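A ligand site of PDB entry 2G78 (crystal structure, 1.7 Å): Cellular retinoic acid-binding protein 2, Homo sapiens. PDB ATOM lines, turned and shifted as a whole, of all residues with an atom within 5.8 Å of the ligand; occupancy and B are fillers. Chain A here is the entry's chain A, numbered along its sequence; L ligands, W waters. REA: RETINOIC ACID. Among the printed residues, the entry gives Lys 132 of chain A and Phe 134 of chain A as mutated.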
ATOM      1  N   PHE A  15      18.680  10.341  -9.754  1.00  0.00           N
ATOM      2  CA  PHE A  15      19.413   9.084 -10.003  1.00  0.00           C
ATOM      3  C   PHE A  15      19.671   8.353  -8.644  1.00  0.00           C
ATOM      4  O   PHE A  15      19.522   7.156  -8.560  1.00  0.00           O
ATOM      5  CB  PHE A  15      20.725   9.336 -10.693  1.00  0.00           C
ATOM      6  CG  PHE A  15      21.477   8.082 -11.102  1.00  0.00           C
ATOM      7  CD1 PHE A  15      20.858   7.056 -11.795  1.00  0.00           C
ATOM      8  CD2 PHE A  15      22.812   7.959 -10.802  1.00  0.00           C
ATOM      9  CE1 PHE A  15      21.545   5.934 -12.176  1.00  0.00           C
ATOM     10  CE2 PHE A  15      23.521   6.789 -11.206  1.00  0.00           C
ATOM     11  CZ  PHE A  15      22.873   5.818 -11.866  1.00  0.00           C
ATOM     12  N   LEU A  19      18.416   4.553  -7.444  1.00  0.00           N
ATOM     13  CA  LEU A  19      19.252   3.467  -6.923  1.00  0.00           C
ATOM     14  C   LEU A  19      18.806   2.998  -5.533  1.00  0.00           C
ATOM     15  O   LEU A  19      18.971   1.807  -5.211  1.00  0.00           O
ATOM     16  CB  LEU A  19      20.709   3.893  -6.904  1.00  0.00           C
ATOM     17  CG  LEU A  19      21.328   4.221  -8.254  1.00  0.00           C
ATOM     18  CD1 LEU A  19      22.751   4.683  -8.002  1.00  0.00           C
ATOM     19  CD2 LEU A  19      21.253   3.057  -9.241  1.00  0.00           C
ATOM     20  N   VAL A  24      20.315  -0.295  -3.611  1.00  0.00           N
ATOM     21  CA  VAL A  24      21.748  -0.097  -3.575  1.00  0.00           C
ATOM     22  C   VAL A  24      22.128   0.674  -2.323  1.00  0.00           C
ATOM     23  O   VAL A  24      21.492   1.708  -2.007  1.00  0.00           O
ATOM     24  CB  VAL A  24      22.231   0.719  -4.826  1.00  0.00           C
ATOM     25  CG1 VAL A  24      23.722   0.862  -4.803  1.00  0.00           C
ATOM     26  CG2 VAL A  24      21.772   0.011  -6.093  1.00  0.00           C
ATOM     27  N   LEU A  28      27.842   2.525  -2.097  1.00  0.00           N
ATOM     28  CA  LEU A  28      27.779   2.137  -3.520  1.00  0.00           C
ATOM     29  C   LEU A  28      27.046   3.232  -4.312  1.00  0.00           C
ATOM     30  O   LEU A  28      27.482   3.586  -5.418  1.00  0.00           O
ATOM     31  CB  LEU A  28      27.064   0.791  -3.729  1.00  0.00           C
ATOM     32  CG  LEU A  28      27.929  -0.401  -3.315  1.00  0.00           C
ATOM     33  CD1 LEU A  28      27.095  -1.682  -3.329  1.00  0.00           C
ATOM     34  CD2 LEU A  28      29.154  -0.529  -4.206  1.00  0.00           C
ATOM     35  N   ILE A  31      29.510   6.019  -5.041  1.00  0.00           N
ATOM     36  CA  ILE A  31      30.355   5.643  -6.163  1.00  0.00           C
ATOM     37  C   ILE A  31      29.575   5.862  -7.485  1.00  0.00           C
ATOM     38  O   ILE A  31      30.079   6.489  -8.416  1.00  0.00           O
ATOM     39  CB  ILE A  31      30.805   4.171  -6.050  1.00  0.00           C
ATOM     40  CG1 ILE A  31      31.794   4.022  -4.887  1.00  0.00           C
ATOM     41  CG2 ILE A  31      31.473   3.722  -7.305  1.00  0.00           C
ATOM     42  CD1 ILE A  31      32.057   2.573  -4.371  1.00  0.00           C
ATOM     43  N   ALA A  32      28.346   5.355  -7.521  1.00  0.00           N
ATOM     44  CA  ALA A  32      27.592   5.293  -8.769  1.00  0.00           C
ATOM     45  C   ALA A  32      27.218   6.708  -9.216  1.00  0.00           C
ATOM     46  O   ALA A  32      27.378   7.082 -10.388  1.00  0.00           O
ATOM     47  CB  ALA A  32      26.377   4.483  -8.572  1.00  0.00           C
ATOM     48  N   VAL A  33      26.733   7.496  -8.265  1.00  0.00           N
ATOM     49  CA  VAL A  33      26.227   8.823  -8.575  1.00  0.00           C
ATOM     50  C   VAL A  33      27.353   9.705  -9.067  1.00  0.00           C
ATOM     51  O   VAL A  33      27.191  10.437 -10.036  1.00  0.00           O
ATOM     52  CB  VAL A  33      25.536   9.393  -7.324  1.00  0.00           C
ATOM     53  CG1 VAL A  33      25.439  10.911  -7.397  1.00  0.00           C
ATOM     54  CG2 VAL A  33      24.155   8.744  -7.146  1.00  0.00           C
ATOM     55  N   ALA A  35      30.170   8.732 -10.594  1.00  0.00           N
ATOM     56  CA  ALA A  35      30.596   8.285 -11.946  1.00  0.00           C
ATOM     57  C   ALA A  35      29.534   8.624 -12.987  1.00  0.00           C
ATOM     58  O   ALA A  35      29.843   9.006 -14.131  1.00  0.00           O
ATOM     59  CB  ALA A  35      30.869   6.795 -11.963  1.00  0.00           C
ATOM     60  N   ALA A  36      28.274   8.490 -12.601  1.00  0.00           N
ATOM     61  CA  ALA A  36      27.194   8.690 -13.561  1.00  0.00           C
ATOM     62  C   ALA A  36      27.067  10.180 -13.896  1.00  0.00           C
ATOM     63  O   ALA A  36      26.359  10.548 -14.849  1.00  0.00           O
ATOM     64  CB  ALA A  36      25.906   8.171 -13.036  1.00  0.00           C
ATOM     65  N   PRO A  39      28.751  10.787 -18.005  1.00  0.00           N
ATOM     66  CA  PRO A  39      28.834   9.603 -18.825  1.00  0.00           C
ATOM     67  C   PRO A  39      29.154  10.000 -20.248  1.00  0.00           C
ATOM     68  O   PRO A  39      29.024  11.187 -20.610  1.00  0.00           O
ATOM     69  CB  PRO A  39      27.430   9.052 -18.751  1.00  0.00           C
ATOM     70  CG  PRO A  39      26.568  10.286 -18.652  1.00  0.00           C
ATOM     71  CD  PRO A  39      27.372  11.268 -17.884  1.00  0.00           C
ATOM     72  N   VAL A  41      27.767   8.760 -24.000  1.00  0.00           N
ATOM     73  CA  VAL A  41      26.678   8.003 -24.572  1.00  0.00           C
ATOM     74  C   VAL A  41      26.833   8.048 -26.074  1.00  0.00           C
ATOM     75  O   VAL A  41      26.789   9.135 -26.653  1.00  0.00           O
ATOM     76  CB  VAL A  41      25.336   8.588 -24.165  1.00  0.00           C
ATOM     77  CG1 VAL A  41      24.253   7.844 -24.837  1.00  0.00           C
ATOM     78  CG2 VAL A  41      25.140   8.472 -22.667  1.00  0.00           C
ATOM     79  N   THR A  54      26.828   3.222 -23.172  1.00  0.00           N
ATOM     80  CA  THR A  54      26.807   4.211 -22.124  1.00  0.00           C
ATOM     81  C   THR A  54      28.002   3.875 -21.233  1.00  0.00           C
ATOM     82  O   THR A  54      28.032   2.815 -20.653  1.00  0.00           O
ATOM     83  CB  THR A  54      25.521   4.138 -21.323  1.00  0.00           C
ATOM     84  OG1 THR A  54      24.384   4.416 -22.187  1.00  0.00           O
ATOM     85  CG2 THR A  54      25.558   5.135 -20.175  1.00  0.00           C
ATOM     86  N   THR A  56      30.807   4.901 -18.169  1.00  0.00           N
ATOM     87  CA  THR A  56      31.258   5.678 -17.008  1.00  0.00           C
ATOM     88  C   THR A  56      32.525   5.011 -16.488  1.00  0.00           C
ATOM     89  O   THR A  56      32.843   3.955 -16.901  1.00  0.00           O
ATOM     90  CB  THR A  56      30.256   5.733 -15.883  1.00  0.00           C
ATOM     91  OG1 THR A  56      30.184   4.448 -15.224  1.00  0.00           O
ATOM     92  CG2 THR A  56      28.886   6.152 -16.426  1.00  0.00           C
ATOM     93  N   VAL A  58      33.027   3.577 -13.810  1.00  0.00           N
ATOM     94  CA  VAL A  58      32.736   2.424 -12.920  1.00  0.00           C
ATOM     95  C   VAL A  58      31.872   1.327 -13.554  1.00  0.00           C
ATOM     96  O   VAL A  58      31.718   0.239 -13.013  1.00  0.00           O
ATOM     97  CB  VAL A  58      32.056   2.828 -11.608  1.00  0.00           C
ATOM     98  CG1 VAL A  58      32.916   3.797 -10.851  1.00  0.00           C
ATOM     99  CG2 VAL A  58      30.658   3.372 -11.854  1.00  0.00           C
ATOM    100  N   ARG A  59      31.304   1.625 -14.724  1.00  0.00           N
ATOM    101  CA  ARG A  59      30.402   0.650 -15.401  1.00  0.00           C
ATOM    102  C   ARG A  59      30.132   1.158 -16.811  1.00  0.00           C
ATOM    103  O   ARG A  59      29.821   2.347 -17.011  1.00  0.00           O
ATOM    104  CB  ARG A  59      29.103   0.494 -14.635  1.00  0.00           C
ATOM    105  CG  ARG A  59      28.036  -0.335 -15.312  1.00  0.00           C
ATOM    106  CD  ARG A  59      26.968  -0.656 -14.327  1.00  0.00           C
ATOM    107  NE  ARG A  59      25.769  -1.222 -14.938  1.00  0.00           N
ATOM    108  CZ  ARG A  59      25.576  -2.513 -15.199  1.00  0.00           C
ATOM    109  NH1 ARG A  59      26.521  -3.441 -14.941  1.00  0.00           N
ATOM    110  NH2 ARG A  59      24.425  -2.891 -15.740  1.00  0.00           N
ATOM    111  N   VAL A  76      19.551  -1.149 -14.249  1.00  0.00           N
ATOM    112  CA  VAL A  76      20.556  -0.173 -13.924  1.00  0.00           C
ATOM    113  C   VAL A  76      21.444  -0.614 -12.766  1.00  0.00           C
ATOM    114  O   VAL A  76      22.627  -0.286 -12.719  1.00  0.00           O
ATOM    115  CB  VAL A  76      19.941   1.231 -13.638  1.00  0.00           C
ATOM    116  CG1 VAL A  76      18.757   1.109 -12.701  1.00  0.00           C
ATOM    117  CG2 VAL A  76      21.020   2.179 -13.064  1.00  0.00           C
ATOM    118  N   ASP A  77      20.900  -1.398 -11.843  1.00  0.00           N
ATOM    119  CA  ASP A  77      21.712  -1.957 -10.741  1.00  0.00           C
ATOM    120  C   ASP A  77      22.346  -3.294 -11.104  1.00  0.00           C
ATOM    121  O   ASP A  77      22.903  -3.957 -10.235  1.00  0.00           O
ATOM    122  CB  ASP A  77      20.870  -2.078  -9.487  1.00  0.00           C
ATOM    123  CG  ASP A  77      19.667  -2.980  -9.656  1.00  0.00           C
ATOM    124  OD1 ASP A  77      18.955  -2.854 -10.703  1.00  0.00           O
ATOM    125  OD2 ASP A  77      19.434  -3.787  -8.728  1.00  0.00           O
ATOM    126  N   ARG A 111      13.495   6.614 -24.085  1.00  0.00           N
ATOM    127  CA  ARG A 111      14.349   7.654 -24.686  1.00  0.00           C
ATOM    128  C   ARG A 111      13.521   8.407 -25.716  1.00  0.00           C
ATOM    129  O   ARG A 111      12.837   7.784 -26.526  1.00  0.00           O
ATOM    130  CB  ARG A 111      15.548   7.012 -25.386  1.00  0.00           C
ATOM    131  CG  ARG A 111      16.633   6.570 -24.400  1.00  0.00           C
ATOM    132  CD  ARG A 111      17.852   5.993 -25.116  1.00  0.00           C
ATOM    133  NE  ARG A 111      18.968   5.773 -24.169  1.00  0.00           N
ATOM    134  CZ  ARG A 111      19.198   4.653 -23.473  1.00  0.00           C
ATOM    135  NH1 ARG A 111      18.423   3.584 -23.576  1.00  0.00           N
ATOM    136  NH2 ARG A 111      20.282   4.584 -22.697  1.00  0.00           N
ATOM    137  N   LEU A 121      16.321  10.793 -21.523  1.00  0.00           N
ATOM    138  CA  LEU A 121      16.305   9.446 -21.009  1.00  0.00           C
ATOM    139  C   LEU A 121      15.554   9.444 -19.679  1.00  0.00           C
ATOM    140  O   LEU A 121      15.767  10.284 -18.832  1.00  0.00           O
ATOM    141  CB  LEU A 121      17.716   8.986 -20.729  1.00  0.00           C
ATOM    142  CG  LEU A 121      17.865   7.714 -19.881  1.00  0.00           C
ATOM    143  CD1 LEU A 121      17.306   6.483 -20.676  1.00  0.00           C
ATOM    144  CD2 LEU A 121      19.302   7.473 -19.458  1.00  0.00           C
ATOM    145  N   MET A 123      14.507   6.551 -16.566  1.00  0.00           N
ATOM    146  CA  MET A 123      14.640   5.239 -15.991  1.00  0.00           C
ATOM    147  C   MET A 123      13.761   5.184 -14.783  1.00  0.00           C
ATOM    148  O   MET A 123      13.825   6.086 -13.921  1.00  0.00           O
ATOM    149  CB  MET A 123      16.085   4.908 -15.624  1.00  0.00           C
ATOM    150  CG  MET A 123      17.054   5.109 -16.764  1.00  0.00           C
ATOM    151  SD  MET A 123      18.748   4.700 -16.314  1.00  0.00           S
ATOM    152  CE  MET A 123      19.189   6.232 -15.591  1.00  0.00           C
ATOM    153  N   LYS A 132      17.278  12.134 -17.291  1.00  0.00           N
ATOM    154  CA  LYS A 132      18.559  12.669 -17.744  1.00  0.00           C
ATOM    155  C   LYS A 132      18.367  13.282 -19.120  1.00  0.00           C
ATOM    156  O   LYS A 132      17.646  12.765 -19.953  1.00  0.00           O
ATOM    157  CB  LYS A 132      19.680  11.626 -17.765  1.00  0.00           C
ATOM    158  CG  LYS A 132      19.993  10.967 -16.433  1.00  0.00           C
ATOM    159  CD  LYS A 132      21.113   9.941 -16.502  1.00  0.00           C
ATOM    160  CE  LYS A 132      21.193   9.258 -15.180  1.00  0.00           C
ATOM    161  NZ  LYS A 132      22.301   8.235 -15.059  1.00  0.00           N
ATOM    162  N   PHE A 134      20.313  15.121 -22.502  1.00  0.00           N
ATOM    163  CA  PHE A 134      21.528  15.192 -23.281  1.00  0.00           C
ATOM    164  C   PHE A 134      21.381  16.074 -24.522  1.00  0.00           C
ATOM    165  O   PHE A 134      20.263  16.251 -25.091  1.00  0.00           O
ATOM    166  CB  PHE A 134      21.978  13.788 -23.766  1.00  0.00           C
ATOM    167  CG  PHE A 134      22.041  12.758 -22.693  1.00  0.00           C
ATOM    168  CD1 PHE A 134      20.875  12.097 -22.228  1.00  0.00           C
ATOM    169  CD2 PHE A 134      23.254  12.367 -22.187  1.00  0.00           C
ATOM    170  CE1 PHE A 134      20.978  11.129 -21.252  1.00  0.00           C
ATOM    171  CE2 PHE A 134      23.350  11.380 -21.252  1.00  0.00           C
ATOM    172  CZ  PHE A 134      22.212  10.788 -20.753  1.00  0.00           C
HETATM  173  C1  REA L   1      28.188   0.265  -9.240  1.00  0.00           C
HETATM  174  C2  REA L   1      27.920  -1.029  -8.479  1.00  0.00           C
HETATM  175  C3  REA L   1      26.760  -0.912  -7.508  1.00  0.00           C
HETATM  176  C4  REA L   1      25.447  -0.570  -8.167  1.00  0.00           C
HETATM  177  C5  REA L   1      25.610   0.556  -9.116  1.00  0.00           C
HETATM  178  C6  REA L   1      26.859   0.849  -9.674  1.00  0.00           C
HETATM  179  C7  REA L   1      27.031   1.845 -10.701  1.00  0.00           C
HETATM  180  C8  REA L   1      26.072   1.918 -11.759  1.00  0.00           C
HETATM  181  C9  REA L   1      26.172   3.047 -12.647  1.00  0.00           C
HETATM  182  C10 REA L   1      25.029   3.246 -13.486  1.00  0.00           C
HETATM  183  C11 REA L   1      25.117   4.199 -14.525  1.00  0.00           C
HETATM  184  C12 REA L   1      23.871   4.312 -15.257  1.00  0.00           C
HETATM  185  C13 REA L   1      23.781   5.257 -16.334  1.00  0.00           C
HETATM  186  C14 REA L   1      22.559   5.206 -17.036  1.00  0.00           C
HETATM  187  C15 REA L   1      22.322   6.088 -18.165  1.00  0.00           C
HETATM  188  C16 REA L   1      29.086   0.051 -10.453  1.00  0.00           C
HETATM  189  C17 REA L   1      28.886   1.304  -8.377  1.00  0.00           C
HETATM  190  C18 REA L   1      24.364   1.292  -9.453  1.00  0.00           C
HETATM  191  C19 REA L   1      27.330   3.991 -12.726  1.00  0.00           C
HETATM  192  C20 REA L   1      24.858   6.224 -16.711  1.00  0.00           C
HETATM  193  O1  REA L   1      22.514   7.333 -18.077  1.00  0.00           O
HETATM  194  O2  REA L   1      22.002   5.556 -19.244  1.00  0.00           O
HETATM  195  O   HOH W   1      24.230   9.449 -16.051  1.00  0.00           O
HETATM  196  O   HOH W   2      22.342   6.278 -21.761  1.00  0.00           O
HETATM  197  O   HOH W   3      22.457   2.859 -19.271  1.00  0.00           O
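CZ of Phe 15 touches C10 of the ligand (3.7 Å).
Leu 19 touches the ligand (CD2 to C18, 3.6 Å).
O of Leu 28 touches C17 of the ligand, 3.99 Å away.
Ile 31 touches the ligand.
Ala 32 touches the ligand.
CG2 of Thr 54 touches C20 of the ligand, 3.7 Å away.
Thr 56 touches the ligand.
CG2 of Val 58 touches C19 of the ligand, at 3.5 Å.
Arg 59 touches the ligand (CD to C8, 3.7 Å).
CD2 of Leu 121 touches O2 of the ligand (3.3 Å).
CE of Met 123 touches C14 of the ligand (3.8 Å).
Hydrophobic or aromatic side chains within 4 Å of the ligand: Phe 15, Leu 19, Ile 31, Ala 32, Val 58, Leu 121 and Met 123.
Of the 22 residues printed, 13 come within 4 Å of the ligand.
An oxygen (O1) of the ligand is in salt-bridge range of the side-chain amino group (NZ) of Lys 132.
The guanidinium group (NH2) of Arg 111 is in salt-bridge range of an oxygen (O2) of the ligand (3.98 Å).
The backbone NH (N) of Lys 132 is in hydrogen-bond range of the backbone carbonyl oxygen (O) of Leu 121 (2.8 Å).
The side-chain hydroxyl (OG1) of Thr 56 sits close to the backbone NH (N) of Val 58 (3.3 Å).
The backbone carbonyl oxygen (O) of Leu 19 sits at hydrogen-bond distance from the backbone NH (N) of Val 24, 3.0 Å away.
The backbone carbonyl oxygen (O) of Arg 59 lies within hydrogen-bond range of the side-chain hydroxyl (OG1) of Thr 56, 2.8 Å away.
Water W2 lies within hydrogen-bond range of an oxygen (O2) of the ligand, the side-chain hydroxyl (OG1) of Thr 54 and the guanidinium group (NH2) of Arg 111.
Water W1 lies within hydrogen-bond range of NZ of Lys 132, O of Ala 36 and O1 of the ligand.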
